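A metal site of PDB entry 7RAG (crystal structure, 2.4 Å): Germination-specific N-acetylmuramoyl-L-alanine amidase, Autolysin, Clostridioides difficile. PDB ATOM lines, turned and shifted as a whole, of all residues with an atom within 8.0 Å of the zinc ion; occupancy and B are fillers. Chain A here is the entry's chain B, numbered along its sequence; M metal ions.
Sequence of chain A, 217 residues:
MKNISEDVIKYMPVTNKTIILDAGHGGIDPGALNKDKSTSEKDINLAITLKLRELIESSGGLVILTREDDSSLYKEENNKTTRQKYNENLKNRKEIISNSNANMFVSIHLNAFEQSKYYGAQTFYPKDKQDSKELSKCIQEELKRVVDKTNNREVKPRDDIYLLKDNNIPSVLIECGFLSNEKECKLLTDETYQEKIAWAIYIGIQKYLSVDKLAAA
Leu 110 touches the zinc ion (O to ZN, 3.9 Å). The nearest printed residue that does not touch the zinc ion is Asn 45 (4.8 Å).
The zinc ion is bound by the side-chain carboxylate of Glu 41 (2.1 Å), a ring nitrogen (NE2) of His 25 (2.3 Å) and a ring nitrogen (ND1) of His 109 (2.3 Å). The zinc ion has three donor atoms within binding distance.
OG of Ser 107 sits close to NE2 of His 109 (3.4 Å). OE2 of Glu 41 lies within hydrogen-bond range of N of Ala 32 (2.6 Å). N of Leu 110 sits close to OE1 of Glu 41 (3.1 Å). O of Ile 174 lies within hydrogen-bond range of N of His 109 (2.9 Å). OD2 of Asp 29 sits at hydrogen-bond distance from ND1 of His 25 (3.1 Å).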
ATOM      1  N   ALA A  23      23.405  13.720 -11.560  1.00  0.00           N
ATOM      2  CA  ALA A  23      22.086  14.270 -11.257  1.00  0.00           C
ATOM      3  C   ALA A  23      21.099  13.602 -12.191  1.00  0.00           C
ATOM      4  O   ALA A  23      21.047  13.919 -13.378  1.00  0.00           O
ATOM      5  CB  ALA A  23      22.051  15.780 -11.418  1.00  0.00           C
ATOM      6  N   GLY A  24      20.340  12.644 -11.682  1.00  0.00           N
ATOM      7  CA  GLY A  24      19.471  11.902 -12.566  1.00  0.00           C
ATOM      8  C   GLY A  24      18.401  12.795 -13.139  1.00  0.00           C
ATOM      9  O   GLY A  24      17.617  13.389 -12.381  1.00  0.00           O
ATOM     10  N   HIS A  25      18.549  13.171 -14.397  1.00  0.00           N
ATOM     11  CA  HIS A  25      17.494  13.252 -15.397  1.00  0.00           C
ATOM     12  C   HIS A  25      18.026  14.414 -16.217  1.00  0.00           C
ATOM     13  O   HIS A  25      19.219  14.716 -16.129  1.00  0.00           O
ATOM     14  CB  HIS A  25      16.077  13.380 -14.835  1.00  0.00           C
ATOM     15  CG  HIS A  25      15.551  12.091 -14.295  1.00  0.00           C
ATOM     16  ND1 HIS A  25      15.243  11.017 -15.101  1.00  0.00           N
ATOM     17  CD2 HIS A  25      15.318  11.678 -13.021  1.00  0.00           C
ATOM     18  CE1 HIS A  25      14.839  10.005 -14.361  1.00  0.00           C
ATOM     19  NE2 HIS A  25      14.879  10.378 -13.086  1.00  0.00           N
ATOM     20  N   ASP A  29      13.579  15.179 -20.168  1.00  0.00           N
ATOM     21  CA  ASP A  29      13.237  14.108 -19.237  1.00  0.00           C
ATOM     22  C   ASP A  29      13.118  14.698 -17.846  1.00  0.00           C
ATOM     23  O   ASP A  29      14.127  14.839 -17.154  1.00  0.00           O
ATOM     24  CB  ASP A  29      14.332  13.029 -19.276  1.00  0.00           C
ATOM     25  CG  ASP A  29      14.040  11.834 -18.349  1.00  0.00           C
ATOM     26  OD1 ASP A  29      12.908  11.714 -17.842  1.00  0.00           O
ATOM     27  OD2 ASP A  29      14.954  11.002 -18.138  1.00  0.00           O
ATOM     28  N   PRO A  30      11.911  15.053 -17.364  1.00  0.00           N
ATOM     29  CA  PRO A  30      11.793  15.365 -15.938  1.00  0.00           C
ATOM     30  C   PRO A  30      11.985  14.070 -15.167  1.00  0.00           C
ATOM     31  O   PRO A  30      12.226  13.022 -15.770  1.00  0.00           O
ATOM     32  CB  PRO A  30      10.378  15.935 -15.821  1.00  0.00           C
ATOM     33  CG  PRO A  30       9.620  15.214 -16.861  1.00  0.00           C
ATOM     34  CD  PRO A  30      10.585  15.045 -18.021  1.00  0.00           C
ATOM     35  N   GLY A  31      11.885  14.084 -13.856  1.00  0.00           N
ATOM     36  CA  GLY A  31      11.862  12.764 -13.270  1.00  0.00           C
ATOM     37  C   GLY A  31      10.452  12.338 -12.948  1.00  0.00           C
ATOM     38  O   GLY A  31       9.560  12.426 -13.789  1.00  0.00           O
ATOM     39  N   ALA A  32      10.253  11.867 -11.728  1.00  0.00           N
ATOM     40  CA  ALA A  32       8.926  11.796 -11.172  1.00  0.00           C
ATOM     41  C   ALA A  32       8.400  13.201 -10.907  1.00  0.00           C
ATOM     42  O   ALA A  32       9.147  14.182 -10.969  1.00  0.00           O
ATOM     43  CB  ALA A  32       8.935  10.994  -9.884  1.00  0.00           C
ATOM     44  N   GLU A  41      11.849  15.830 -10.565  1.00  0.00           N
ATOM     45  CA  GLU A  41      13.145  15.328 -10.088  1.00  0.00           C
ATOM     46  C   GLU A  41      14.305  16.149 -10.637  1.00  0.00           C
ATOM     47  O   GLU A  41      15.231  16.484  -9.893  1.00  0.00           O
ATOM     48  CB  GLU A  41      13.349  13.873 -10.490  1.00  0.00           C
ATOM     49  CG  GLU A  41      12.735  12.810  -9.616  1.00  0.00           C
ATOM     50  CD  GLU A  41      13.121  11.416 -10.091  1.00  0.00           C
ATOM     51  OE1 GLU A  41      14.334  11.100 -10.084  1.00  0.00           O
ATOM     52  OE2 GLU A  41      12.227  10.647 -10.490  1.00  0.00           O
ATOM     53  N   LYS A  42      14.290  16.475 -11.939  1.00  0.00           N
ATOM     54  CA  LYS A  42      15.405  17.126 -12.629  1.00  0.00           C
ATOM     55  C   LYS A  42      16.119  18.169 -11.767  1.00  0.00           C
ATOM     56  O   LYS A  42      17.320  18.050 -11.470  1.00  0.00           O
ATOM     57  CB  LYS A  42      14.906  17.860 -13.880  1.00  0.00           C
ATOM     58  CG  LYS A  42      14.579  17.016 -15.068  1.00  0.00           C
ATOM     59  CD  LYS A  42      14.531  17.880 -16.361  1.00  0.00           C
ATOM     60  CE  LYS A  42      13.815  19.212 -16.168  1.00  0.00           C
ATOM     61  NZ  LYS A  42      13.695  19.964 -17.461  1.00  0.00           N
ATOM     62  N   ASN A  45      17.392  17.070  -8.159  1.00  0.00           N
ATOM     63  CA  ASN A  45      18.588  16.253  -8.307  1.00  0.00           C
ATOM     64  C   ASN A  45      19.800  17.120  -8.618  1.00  0.00           C
ATOM     65  O   ASN A  45      20.874  16.957  -8.017  1.00  0.00           O
ATOM     66  CB  ASN A  45      18.400  15.216  -9.419  1.00  0.00           C
ATOM     67  CG  ASN A  45      17.372  14.173  -9.095  1.00  0.00           C
ATOM     68  OD1 ASN A  45      16.904  14.067  -7.969  1.00  0.00           O
ATOM     69  ND2 ASN A  45      17.015  13.392 -10.098  1.00  0.00           N
ATOM     70  N   TYR A  86      16.125   8.908 -24.198  1.00  0.00           N
ATOM     71  CA  TYR A  86      16.441   8.396 -22.879  1.00  0.00           C
ATOM     72  C   TYR A  86      17.574   7.369 -22.930  1.00  0.00           C
ATOM     73  O   TYR A  86      18.519   7.429 -22.119  1.00  0.00           O
ATOM     74  CB  TYR A  86      15.168   7.787 -22.292  1.00  0.00           C
ATOM     75  CG  TYR A  86      15.276   7.161 -20.923  1.00  0.00           C
ATOM     76  CD1 TYR A  86      15.121   7.923 -19.776  1.00  0.00           C
ATOM     77  CD2 TYR A  86      15.473   5.795 -20.770  1.00  0.00           C
ATOM     78  CE1 TYR A  86      15.200   7.351 -18.525  1.00  0.00           C
ATOM     79  CE2 TYR A  86      15.552   5.211 -19.527  1.00  0.00           C
ATOM     80  CZ  TYR A  86      15.422   5.997 -18.403  1.00  0.00           C
ATOM     81  OH  TYR A  86      15.495   5.406 -17.161  1.00  0.00           O
ATOM     82  N   SER A 107      24.897   8.515  -7.863  1.00  0.00           N
ATOM     83  CA  SER A 107      23.758   8.966  -8.643  1.00  0.00           C
ATOM     84  C   SER A 107      22.692   9.487  -7.680  1.00  0.00           C
ATOM     85  O   SER A 107      22.397   8.842  -6.671  1.00  0.00           O
ATOM     86  CB  SER A 107      23.211   7.825  -9.481  1.00  0.00           C
ATOM     87  OG  SER A 107      22.163   8.287 -10.299  1.00  0.00           O
ATOM     88  N   ILE A 108      22.154  10.674  -7.980  1.00  0.00           N
ATOM     89  CA  ILE A 108      21.159  11.349  -7.131  1.00  0.00           C
ATOM     90  C   ILE A 108      19.822  11.386  -7.881  1.00  0.00           C
ATOM     91  O   ILE A 108      19.705  12.060  -8.917  1.00  0.00           O
ATOM     92  CB  ILE A 108      21.606  12.772  -6.767  1.00  0.00           C
ATOM     93  CG1 ILE A 108      23.017  12.789  -6.172  1.00  0.00           C
ATOM     94  CG2 ILE A 108      20.543  13.443  -5.875  1.00  0.00           C
ATOM     95  CD1 ILE A 108      23.083  12.213  -4.801  1.00  0.00           C
ATOM     96  N   HIS A 109      18.814  10.702  -7.330  1.00  0.00           N
ATOM     97  CA  HIS A 109      17.459  10.674  -7.856  1.00  0.00           C
ATOM     98  C   HIS A 109      16.468  10.998  -6.737  1.00  0.00           C
ATOM     99  O   HIS A 109      16.848  11.339  -5.610  1.00  0.00           O
ATOM    100  CB  HIS A 109      17.116   9.307  -8.491  1.00  0.00           C
ATOM    101  CG  HIS A 109      17.754   9.074  -9.832  1.00  0.00           C
ATOM    102  ND1 HIS A 109      17.020   8.994 -10.990  1.00  0.00           N
ATOM    103  CD2 HIS A 109      19.045   8.898 -10.184  1.00  0.00           C
ATOM    104  CE1 HIS A 109      17.837   8.772 -12.010  1.00  0.00           C
ATOM    105  NE2 HIS A 109      19.063   8.711 -11.545  1.00  0.00           N
ATOM    106  N   LEU A 110      15.181  10.902  -7.058  1.00  0.00           N
ATOM    107  CA  LEU A 110      14.100  10.932  -6.075  1.00  0.00           C
ATOM    108  C   LEU A 110      13.109   9.856  -6.476  1.00  0.00           C
ATOM    109  O   LEU A 110      13.123   9.346  -7.595  1.00  0.00           O
ATOM    110  CB  LEU A 110      13.388  12.296  -6.033  1.00  0.00           C
ATOM    111  CG  LEU A 110      14.162  13.615  -6.026  1.00  0.00           C
ATOM    112  CD1 LEU A 110      13.210  14.752  -6.300  1.00  0.00           C
ATOM    113  CD2 LEU A 110      14.863  13.827  -4.686  1.00  0.00           C
ATOM    114  N   ASN A 111      12.220   9.517  -5.547  1.00  0.00           N
ATOM    115  CA  ASN A 111      11.212   8.490  -5.803  1.00  0.00           C
ATOM    116  C   ASN A 111       9.831   9.128  -5.813  1.00  0.00           C
ATOM    117  O   ASN A 111       9.646  10.261  -5.375  1.00  0.00           O
ATOM    118  CB  ASN A 111      11.298   7.381  -4.755  1.00  0.00           C
ATOM    119  CG  ASN A 111      10.837   6.027  -5.298  1.00  0.00           C
ATOM    120  OD1 ASN A 111      10.468   5.902  -6.469  1.00  0.00           O
ATOM    121  ND2 ASN A 111      10.872   4.997  -4.445  1.00  0.00           N
ATOM    122  N   ALA A 112       8.859   8.371  -6.321  1.00  0.00           N
ATOM    123  CA  ALA A 112       7.446   8.758  -6.236  1.00  0.00           C
ATOM    124  C   ALA A 112       6.589   7.528  -6.479  1.00  0.00           C
ATOM    125  O   ALA A 112       6.730   6.875  -7.522  1.00  0.00           O
ATOM    126  CB  ALA A 112       7.088   9.862  -7.233  1.00  0.00           C
ATOM    127  N   LEU A 173      23.256   4.500  -5.730  1.00  0.00           N
ATOM    128  CA  LEU A 173      22.176   5.395  -6.103  1.00  0.00           C
ATOM    129  C   LEU A 173      21.510   5.870  -4.834  1.00  0.00           C
ATOM    130  O   LEU A 173      21.261   5.076  -3.933  1.00  0.00           O
ATOM    131  CB  LEU A 173      21.158   4.689  -6.995  1.00  0.00           C
ATOM    132  CG  LEU A 173      19.871   5.494  -7.250  1.00  0.00           C
ATOM    133  CD1 LEU A 173      20.129   6.363  -8.442  1.00  0.00           C
ATOM    134  CD2 LEU A 173      18.644   4.610  -7.487  1.00  0.00           C
ATOM    135  N   ILE A 174      21.193   7.165  -4.755  1.00  0.00           N
ATOM    136  CA  ILE A 174      20.495   7.711  -3.605  1.00  0.00           C
ATOM    137  C   ILE A 174      19.195   8.336  -4.076  1.00  0.00           C
ATOM    138  O   ILE A 174      19.208   9.305  -4.850  1.00  0.00           O
ATOM    139  CB  ILE A 174      21.350   8.741  -2.859  1.00  0.00           C
ATOM    140  CG1 ILE A 174      22.757   8.208  -2.650  1.00  0.00           C
ATOM    141  CG2 ILE A 174      20.716   9.051  -1.521  1.00  0.00           C
ATOM    142  CD1 ILE A 174      23.587   9.119  -1.881  1.00  0.00           C
ATOM    143  N   GLU A 175      18.076   7.804  -3.589  1.00  0.00           N
ATOM    144  CA  GLU A 175      16.764   8.413  -3.781  1.00  0.00           C
ATOM    145  C   GLU A 175      16.453   9.232  -2.534  1.00  0.00           C
ATOM    146  O   GLU A 175      16.119   8.678  -1.485  1.00  0.00           O
ATOM    147  CB  GLU A 175      15.701   7.348  -4.023  1.00  0.00           C
ATOM    148  CG  GLU A 175      15.908   6.677  -5.342  1.00  0.00           C
ATOM    149  CD  GLU A 175      14.761   5.790  -5.735  1.00  0.00           C
ATOM    150  OE1 GLU A 175      13.837   5.586  -4.907  1.00  0.00           O
ATOM    151  OE2 GLU A 175      14.809   5.300  -6.897  1.00  0.00           O
HETATM  152 ZN    ZN M   1      14.777   9.302 -11.099  1.00  0.00          ZN
